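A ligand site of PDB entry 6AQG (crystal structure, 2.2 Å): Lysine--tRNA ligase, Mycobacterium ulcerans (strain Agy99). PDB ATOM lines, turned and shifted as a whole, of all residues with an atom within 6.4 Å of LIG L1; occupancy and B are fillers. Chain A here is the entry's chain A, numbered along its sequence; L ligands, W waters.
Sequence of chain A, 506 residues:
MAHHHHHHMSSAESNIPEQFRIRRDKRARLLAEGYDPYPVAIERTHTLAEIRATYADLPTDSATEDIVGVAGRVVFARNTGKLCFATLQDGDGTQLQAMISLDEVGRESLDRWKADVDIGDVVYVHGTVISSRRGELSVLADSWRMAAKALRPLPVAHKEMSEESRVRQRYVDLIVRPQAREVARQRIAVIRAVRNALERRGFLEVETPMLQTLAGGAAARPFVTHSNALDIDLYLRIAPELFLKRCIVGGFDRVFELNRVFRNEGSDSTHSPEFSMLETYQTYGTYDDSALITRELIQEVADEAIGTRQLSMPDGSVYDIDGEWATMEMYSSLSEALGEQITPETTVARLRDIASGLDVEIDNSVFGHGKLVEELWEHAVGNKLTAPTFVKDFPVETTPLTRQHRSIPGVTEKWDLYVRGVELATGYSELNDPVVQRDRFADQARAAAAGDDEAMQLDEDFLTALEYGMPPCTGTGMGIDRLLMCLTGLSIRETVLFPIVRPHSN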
ATOM      1  N   GLY A 217       2.389  12.982 -20.105  1.00  0.00           N
ATOM      2  CA  GLY A 217       3.445  13.890 -19.692  1.00  0.00           C
ATOM      3  C   GLY A 217       4.088  14.693 -20.803  1.00  0.00           C
ATOM      4  O   GLY A 217       4.969  15.533 -20.533  1.00  0.00           O
ATOM      5  N   ALA A 218       3.720  14.442 -22.058  1.00  0.00           N
ATOM      6  CA  ALA A 218       4.216  15.211 -23.190  1.00  0.00           C
ATOM      7  C   ALA A 218       3.225  15.010 -24.320  1.00  0.00           C
ATOM      8  O   ALA A 218       2.232  14.287 -24.187  1.00  0.00           O
ATOM      9  CB  ALA A 218       5.631  14.782 -23.604  1.00  0.00           C
ATOM     10  N   ALA A 219       3.487  15.658 -25.442  1.00  0.00           N
ATOM     11  CA  ALA A 219       2.667  15.532 -26.635  1.00  0.00           C
ATOM     12  C   ALA A 219       3.508  14.835 -27.694  1.00  0.00           C
ATOM     13  O   ALA A 219       4.351  15.470 -28.349  1.00  0.00           O
ATOM     14  CB  ALA A 219       2.178  16.915 -27.098  1.00  0.00           C
ATOM     15  N   ILE A 238       6.968   8.518 -22.921  1.00  0.00           N
ATOM     16  CA  ILE A 238       7.391   9.736 -23.611  1.00  0.00           C
ATOM     17  C   ILE A 238       7.901  10.793 -22.638  1.00  0.00           C
ATOM     18  O   ILE A 238       8.549  11.759 -23.078  1.00  0.00           O
ATOM     19  CB  ILE A 238       6.234  10.319 -24.460  1.00  0.00           C
ATOM     20  CG1 ILE A 238       5.027  10.636 -23.571  1.00  0.00           C
ATOM     21  CG2 ILE A 238       5.822   9.313 -25.535  1.00  0.00           C
ATOM     22  CD1 ILE A 238       3.828  11.247 -24.338  1.00  0.00           C
ATOM     23  N   ALA A 239       7.641  10.635 -21.332  1.00  0.00           N
ATOM     24  CA  ALA A 239       8.145  11.536 -20.286  1.00  0.00           C
ATOM     25  C   ALA A 239       7.932  10.894 -18.922  1.00  0.00           C
ATOM     26  O   ALA A 239       7.006  10.086 -18.768  1.00  0.00           O
ATOM     27  CB  ALA A 239       7.455  12.909 -20.338  1.00  0.00           C
ATOM     28  N   PRO A 240       8.749  11.226 -17.923  1.00  0.00           N
ATOM     29  CA  PRO A 240       8.489  10.767 -16.536  1.00  0.00           C
ATOM     30  C   PRO A 240       7.582  11.675 -15.705  1.00  0.00           C
ATOM     31  O   PRO A 240       7.304  11.336 -14.550  1.00  0.00           O
ATOM     32  CB  PRO A 240       9.896  10.730 -15.929  1.00  0.00           C
ATOM     33  CG  PRO A 240      10.595  11.941 -16.619  1.00  0.00           C
ATOM     34  CD  PRO A 240      10.069  11.900 -18.052  1.00  0.00           C
ATOM     35  N   GLU A 241       7.088  12.769 -16.305  1.00  0.00           N
ATOM     36  CA  GLU A 241       6.421  13.847 -15.550  1.00  0.00           C
ATOM     37  C   GLU A 241       5.284  13.349 -14.616  1.00  0.00           C
ATOM     38  O   GLU A 241       5.199  13.758 -13.444  1.00  0.00           O
ATOM     39  CB  GLU A 241       5.886  14.875 -16.546  1.00  0.00           C
ATOM     40  CG  GLU A 241       4.821  15.798 -15.952  1.00  0.00           C
ATOM     41  CD  GLU A 241       4.735  17.179 -16.619  1.00  0.00           C
ATOM     42  OE1 GLU A 241       5.436  17.441 -17.639  1.00  0.00           O
ATOM     43  OE2 GLU A 241       3.962  18.026 -16.103  1.00  0.00           O
ATOM     44  N   LYS A 245       5.413  13.615 -10.511  1.00  0.00           N
ATOM     45  CA  LYS A 245       4.447  14.358  -9.710  1.00  0.00           C
ATOM     46  C   LYS A 245       3.828  13.480  -8.624  1.00  0.00           C
ATOM     47  O   LYS A 245       3.537  13.982  -7.529  1.00  0.00           O
ATOM     48  CB  LYS A 245       3.344  14.953 -10.595  1.00  0.00           C
ATOM     49  CG  LYS A 245       3.901  16.118 -11.419  1.00  0.00           C
ATOM     50  CD  LYS A 245       2.861  16.619 -12.429  1.00  0.00           C
ATOM     51  CE  LYS A 245       3.115  18.109 -12.697  1.00  0.00           C
ATOM     52  NZ  LYS A 245       2.499  18.567 -13.950  1.00  0.00           N
ATOM     53  N   ARG A 263      10.079   8.720 -28.113  1.00  0.00           N
ATOM     54  CA  ARG A 263       8.987   9.356 -28.858  1.00  0.00           C
ATOM     55  C   ARG A 263       8.992   8.862 -30.291  1.00  0.00           C
ATOM     56  O   ARG A 263      10.019   8.924 -30.986  1.00  0.00           O
ATOM     57  CB  ARG A 263       9.078  10.885 -28.761  1.00  0.00           C
ATOM     58  CG  ARG A 263       9.242  11.356 -27.285  1.00  0.00           C
ATOM     59  CD  ARG A 263       8.948  12.832 -27.043  1.00  0.00           C
ATOM     60  NE  ARG A 263       9.048  13.132 -25.613  1.00  0.00           N
ATOM     61  CZ  ARG A 263       9.053  14.358 -25.108  1.00  0.00           C
ATOM     62  NH1 ARG A 263       8.954  15.417 -25.906  1.00  0.00           N
ATOM     63  NH2 ARG A 263       9.159  14.538 -23.784  1.00  0.00           N
ATOM     64  N   LEU A 278      16.477  15.242 -18.760  1.00  0.00           N
ATOM     65  CA  LEU A 278      16.409  15.528 -17.336  1.00  0.00           C
ATOM     66  C   LEU A 278      15.038  16.131 -17.013  1.00  0.00           C
ATOM     67  O   LEU A 278      14.554  17.001 -17.736  1.00  0.00           O
ATOM     68  CB  LEU A 278      17.504  16.530 -16.955  1.00  0.00           C
ATOM     69  CG  LEU A 278      17.393  17.152 -15.558  1.00  0.00           C
ATOM     70  CD1 LEU A 278      17.753  16.135 -14.494  1.00  0.00           C
ATOM     71  CD2 LEU A 278      18.304  18.373 -15.465  1.00  0.00           C
ATOM     72  N   GLU A 279      14.407  15.664 -15.927  1.00  0.00           N
ATOM     73  CA  GLU A 279      13.256  16.362 -15.371  1.00  0.00           C
ATOM     74  C   GLU A 279      13.488  16.568 -13.876  1.00  0.00           C
ATOM     75  O   GLU A 279      13.952  15.654 -13.200  1.00  0.00           O
ATOM     76  CB  GLU A 279      11.926  15.616 -15.588  1.00  0.00           C
ATOM     77  CG  GLU A 279      11.316  15.767 -17.000  1.00  0.00           C
ATOM     78  CD  GLU A 279       9.835  15.338 -17.064  1.00  0.00           C
ATOM     79  OE1 GLU A 279       9.190  15.316 -15.992  1.00  0.00           O
ATOM     80  OE2 GLU A 279       9.309  15.064 -18.167  1.00  0.00           O
ATOM     81  N   THR A 280      13.193  17.781 -13.379  1.00  0.00           N
ATOM     82  CA  THR A 280      13.344  18.120 -11.969  1.00  0.00           C
ATOM     83  C   THR A 280      12.022  18.656 -11.413  1.00  0.00           C
ATOM     84  O   THR A 280      11.240  19.279 -12.142  1.00  0.00           O
ATOM     85  CB  THR A 280      14.439  19.208 -11.736  1.00  0.00           C
ATOM     86  OG1 THR A 280      13.952  20.476 -12.163  1.00  0.00           O
ATOM     87  CG2 THR A 280      15.743  18.885 -12.468  1.00  0.00           C
ATOM     88  N   TYR A 281      11.764  18.392 -10.122  1.00  0.00           N
ATOM     89  CA  TYR A 281      10.582  18.959  -9.451  1.00  0.00           C
ATOM     90  C   TYR A 281      10.995  19.485  -8.087  1.00  0.00           C
ATOM     91  O   TYR A 281      11.783  18.856  -7.384  1.00  0.00           O
ATOM     92  CB  TYR A 281       9.416  17.935  -9.365  1.00  0.00           C
ATOM     93  CG  TYR A 281       8.871  17.671 -10.752  1.00  0.00           C
ATOM     94  CD1 TYR A 281       9.506  16.795 -11.617  1.00  0.00           C
ATOM     95  CD2 TYR A 281       7.785  18.386 -11.241  1.00  0.00           C
ATOM     96  CE1 TYR A 281       9.067  16.625 -12.930  1.00  0.00           C
ATOM     97  CE2 TYR A 281       7.320  18.194 -12.539  1.00  0.00           C
ATOM     98  CZ  TYR A 281       7.977  17.316 -13.385  1.00  0.00           C
ATOM     99  OH  TYR A 281       7.536  17.143 -14.676  1.00  0.00           O
ATOM    100  N   LEU A 401      -0.725  20.886 -18.660  1.00  0.00           N
ATOM    101  CA  LEU A 401      -0.223  20.501 -17.347  1.00  0.00           C
ATOM    102  C   LEU A 401       0.338  21.690 -16.572  1.00  0.00           C
ATOM    103  O   LEU A 401       0.895  21.510 -15.486  1.00  0.00           O
ATOM    104  CB  LEU A 401       0.814  19.385 -17.500  1.00  0.00           C
ATOM    105  CG  LEU A 401       0.279  18.077 -18.137  1.00  0.00           C
ATOM    106  CD1 LEU A 401       1.386  17.023 -18.370  1.00  0.00           C
ATOM    107  CD2 LEU A 401      -0.823  17.447 -17.310  1.00  0.00           C
ATOM    108  N   GLU A 423      15.830  24.786 -28.933  1.00  0.00           N
ATOM    109  CA  GLU A 423      14.921  24.677 -27.791  1.00  0.00           C
ATOM    110  C   GLU A 423      15.515  23.689 -26.791  1.00  0.00           C
ATOM    111  O   GLU A 423      15.543  22.481 -27.045  1.00  0.00           O
ATOM    112  CB  GLU A 423      13.524  24.247 -28.256  1.00  0.00           C
ATOM    113  CG  GLU A 423      12.596  23.867 -27.072  1.00  0.00           C
ATOM    114  CD  GLU A 423      11.236  23.269 -27.513  1.00  0.00           C
ATOM    115  OE1 GLU A 423      10.900  23.267 -28.729  1.00  0.00           O
ATOM    116  OE2 GLU A 423      10.491  22.807 -26.617  1.00  0.00           O
ATOM    117  N   THR A 426      12.516  23.710 -20.511  1.00  0.00           N
ATOM    118  CA  THR A 426      11.218  24.311 -20.248  1.00  0.00           C
ATOM    119  C   THR A 426      10.959  24.180 -18.749  1.00  0.00           C
ATOM    120  O   THR A 426      11.500  23.298 -18.101  1.00  0.00           O
ATOM    121  CB  THR A 426      10.117  23.637 -21.102  1.00  0.00           C
ATOM    122  OG1 THR A 426       8.904  24.381 -20.990  1.00  0.00           O
ATOM    123  CG2 THR A 426       9.871  22.190 -20.658  1.00  0.00           C
ATOM    124  N   GLY A 427      10.180  25.110 -18.206  1.00  0.00           N
ATOM    125  CA  GLY A 427       9.776  25.037 -16.803  1.00  0.00           C
ATOM    126  C   GLY A 427       8.362  25.538 -16.593  1.00  0.00           C
ATOM    127  O   GLY A 427       7.908  26.475 -17.257  1.00  0.00           O
ATOM    128  N   TYR A 428       7.667  24.918 -15.635  1.00  0.00           N
ATOM    129  CA  TYR A 428       6.288  25.280 -15.291  1.00  0.00           C
ATOM    130  C   TYR A 428       6.164  25.630 -13.808  1.00  0.00           C
ATOM    131  O   TYR A 428       6.854  25.070 -12.968  1.00  0.00           O
ATOM    132  CB  TYR A 428       5.271  24.133 -15.512  1.00  0.00           C
ATOM    133  CG  TYR A 428       5.209  23.389 -16.837  1.00  0.00           C
ATOM    134  CD1 TYR A 428       5.846  23.856 -17.995  1.00  0.00           C
ATOM    135  CD2 TYR A 428       4.484  22.190 -16.922  1.00  0.00           C
ATOM    136  CE1 TYR A 428       5.777  23.129 -19.214  1.00  0.00           C
ATOM    137  CE2 TYR A 428       4.391  21.461 -18.116  1.00  0.00           C
ATOM    138  CZ  TYR A 428       5.035  21.934 -19.259  1.00  0.00           C
ATOM    139  OH  TYR A 428       4.943  21.198 -20.422  1.00  0.00           O
ATOM    140  N   GLU A 430       3.579  24.257 -11.588  1.00  0.00           N
ATOM    141  CA  GLU A 430       2.833  23.036 -11.907  1.00  0.00           C
ATOM    142  C   GLU A 430       1.365  23.193 -11.553  1.00  0.00           C
ATOM    143  O   GLU A 430       1.018  23.733 -10.498  1.00  0.00           O
ATOM    144  CB  GLU A 430       3.417  21.826 -11.166  1.00  0.00           C
ATOM    145  CG  GLU A 430       4.888  21.447 -11.594  1.00  0.00           C
ATOM    146  CD  GLU A 430       5.062  21.189 -13.100  1.00  0.00           C
ATOM    147  OE1 GLU A 430       6.212  21.298 -13.599  1.00  0.00           O
ATOM    148  OE2 GLU A 430       4.076  20.851 -13.807  1.00  0.00           O
ATOM    149  N   THR A 474       7.409  23.537  -8.836  1.00  0.00           N
ATOM    150  CA  THR A 474       7.835  23.879 -10.177  1.00  0.00           C
ATOM    151  C   THR A 474       8.679  22.750 -10.743  1.00  0.00           C
ATOM    152  O   THR A 474       9.568  22.220 -10.055  1.00  0.00           O
ATOM    153  CB  THR A 474       8.594  25.231 -10.217  1.00  0.00           C
ATOM    154  OG1 THR A 474       8.992  25.487 -11.568  1.00  0.00           O
ATOM    155  CG2 THR A 474       9.855  25.244  -9.346  1.00  0.00           C
ATOM    156  N   GLY A 475       8.403  22.386 -11.996  1.00  0.00           N
ATOM    157  CA  GLY A 475       9.135  21.345 -12.680  1.00  0.00           C
ATOM    158  C   GLY A 475       9.867  21.888 -13.901  1.00  0.00           C
ATOM    159  O   GLY A 475       9.450  22.879 -14.504  1.00  0.00           O
ATOM    160  N   THR A 476      10.961  21.226 -14.263  1.00  0.00           N
ATOM    161  CA  THR A 476      11.689  21.547 -15.486  1.00  0.00           C
ATOM    162  C   THR A 476      11.950  20.283 -16.301  1.00  0.00           C
ATOM    163  O   THR A 476      11.994  19.161 -15.778  1.00  0.00           O
ATOM    164  CB  THR A 476      13.060  22.238 -15.215  1.00  0.00           C
ATOM    165  OG1 THR A 476      13.992  21.305 -14.669  1.00  0.00           O
ATOM    166  CG2 THR A 476      12.911  23.460 -14.255  1.00  0.00           C
ATOM    167  N   GLY A 477      12.157  20.487 -17.597  1.00  0.00           N
ATOM    168  CA  GLY A 477      12.611  19.425 -18.474  1.00  0.00           C
ATOM    169  C   GLY A 477      13.725  19.961 -19.346  1.00  0.00           C
ATOM    170  O   GLY A 477      13.693  21.109 -19.762  1.00  0.00           O
ATOM    171  N   MET A 478      14.714  19.113 -19.603  1.00  0.00           N
ATOM    172  CA  MET A 478      15.835  19.522 -20.435  1.00  0.00           C
ATOM    173  C   MET A 478      16.326  18.334 -21.252  1.00  0.00           C
ATOM    174  O   MET A 478      16.533  17.255 -20.693  1.00  0.00           O
ATOM    175  CB  MET A 478      16.971  20.114 -19.588  1.00  0.00           C
ATOM    176  CG  MET A 478      18.165  20.569 -20.475  1.00  0.00           C
ATOM    177  SD  MET A 478      19.364  21.596 -19.590  1.00  0.00           S
ATOM    178  CE  MET A 478      20.010  20.404 -18.461  1.00  0.00           C
HETATM  179  N1  LIG L   1       7.353  16.597 -19.549  1.00  0.00           N
HETATM  180  C1  LIG L   1       7.935  17.803 -20.142  1.00  0.00           C
HETATM  181  C2  LIG L   1       8.295  17.535 -21.612  1.00  0.00           C
HETATM  182  O1  LIG L   1       8.499  16.355 -21.992  1.00  0.00           O
HETATM  183  C3  LIG L   1       9.168  18.256 -19.345  1.00  0.00           C
HETATM  184  C4  LIG L   1       8.800  18.767 -17.952  1.00  0.00           C
HETATM  185  C5  LIG L   1       7.754  19.870 -18.098  1.00  0.00           C
HETATM  186  C6  LIG L   1       7.613  20.596 -16.742  1.00  0.00           C
HETATM  187  N2  LIG L   1       6.778  19.830 -15.825  1.00  0.00           N
HETATM  188  O2  LIG L   1       8.392  18.476 -22.440  1.00  0.00           O
HETATM  189  O1  LG2 L   2      15.996  16.227 -27.923  1.00  0.00           O
HETATM  190  C1  LG2 L   2      14.804  16.391 -27.842  1.00  0.00           C
HETATM  191  C2  LG2 L   2      13.773  15.631 -28.594  1.00  0.00           C
HETATM  192  C3  LG2 L   2      12.437  16.012 -28.538  1.00  0.00           C
HETATM  193  C4  LG2 L   2      11.462  15.334 -29.214  1.00  0.00           C
HETATM  194  C5  LG2 L   2      11.802  14.232 -29.980  1.00  0.00           C
HETATM  195  O2  LG2 L   2      10.832  13.541 -30.654  1.00  0.00           O
HETATM  196  C6  LG2 L   2      13.132  13.820 -30.054  1.00  0.00           C
HETATM  197  C7  LG2 L   2      14.134  14.510 -29.374  1.00  0.00           C
HETATM  198  O3  LG2 L   2      15.446  14.138 -29.445  1.00  0.00           O
HETATM  199  O4  LG2 L   2      14.343  17.334 -26.929  1.00  0.00           O
HETATM  200  C8  LG2 L   2      12.951  17.536 -26.549  1.00  0.00           C
HETATM  201  C9  LG2 L   2      12.014  17.220 -27.720  1.00  0.00           C
HETATM  202  C10 LG2 L   2      12.679  18.939 -25.990  1.00  0.00           C
HETATM  203  C11 LG2 L   2      13.623  19.294 -24.832  1.00  0.00           C
HETATM  204  O5  LG2 L   2      13.472  18.134 -23.950  1.00  0.00           O
HETATM  205  C12 LG2 L   2      12.336  18.001 -23.057  1.00  0.00           C
HETATM  206  C13 LG2 L   2      12.548  16.815 -22.081  1.00  0.00           C
HETATM  207  C14 LG2 L   2      12.021  19.337 -22.331  1.00  0.00           C
HETATM  208  C15 LG2 L   2      12.041  20.558 -23.263  1.00  0.00           C
HETATM  209  C16 LG2 L   2      13.330  20.630 -24.110  1.00  0.00           C
HETATM  210  O   HOH W   1      10.356  14.241 -20.847  1.00  0.00           O
HETATM  211  O   HOH W   2       8.729  18.026 -24.860  1.00  0.00           O
HETATM  212  O   HOH W   3       7.335  20.927 -22.546  1.00  0.00           O
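OE1 of Glu 430 sits at hydrogen-bond distance from N of Gly 475, at 2.9 Å. The side-chain carboxylate (OE2) of Glu 430 is in salt-bridge range of the side-chain amino group (NZ) of Lys 245, 2.8 Å away. The backbone NH (N) of Glu 241 sits close to the side-chain carboxylate (OE1) of Glu 279, 3.3 Å away. The side-chain carboxylate (OE2) of Glu 241 lies within salt-bridge range of the side-chain amino group (NZ) of Lys 245 (2.7 Å). The side-chain carboxylate (OE1) of Glu 279 sits at hydrogen-bond distance from the side-chain hydroxyl (OH) of Tyr 281, at 2.8 Å. O of Tyr 428 is in hydrogen-bond range of OG1 of Thr 474, at 2.6 Å. The backbone carbonyl oxygen (O) of Thr 426 sits at hydrogen-bond distance from the backbone NH (N) of Gly 477. OG1 of Thr 476 sits at hydrogen-bond distance from OG1 of Thr 280 (2.6 Å).
The guanidinium group of Arg 263 lies within salt-bridge range of an oxygen (O1) of LIG L1. N2 of LIG L1 lies within salt-bridge range of OE1 of Glu 430 (2.7 Å). N1 of LIG L1 sits at hydrogen-bond distance from O of Gly 217, 2.8 Å away. The side-chain carboxylate of Glu 241 is in salt-bridge range of a nitrogen (N1) of LIG L1. OE2 of Glu 279 is in salt-bridge range of N1 of LIG L1 (2.8 Å). N2 of LIG L1 is in hydrogen-bond range of OH of Tyr 281.
Merely in contact with LIG L1: Ala 218 (3.6 Å), Ala 239 (3.8 Å), Tyr 428 (3.5 Å), Gly 475 (3.7 Å), Thr 476 (3.9 Å) and Gly 477 (3.7 Å). Hydrophobic or aromatic side chains within 4 Å of LIG L1: Ala 218, Ala 239, Tyr 281 and Tyr 428. The nearest printed residue that does not touch LIG L1 is Thr 426 (4.1 Å).
Water W2 lies within hydrogen-bond range of an oxygen (O2) of LIG L1 and the guanidinium group (NH1) of Arg 263. Water W3 bridges an oxygen (O2) of LIG L1 (2.7 Å) and the side-chain hydroxyl of Tyr 428 (3.2 Å). Water W1 lies within hydrogen-bond range of OE2 of Glu 279 (3.0 Å), O1 of LIG L1 (3.0 Å) and NH2 of Arg 263 (3.2 Å).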
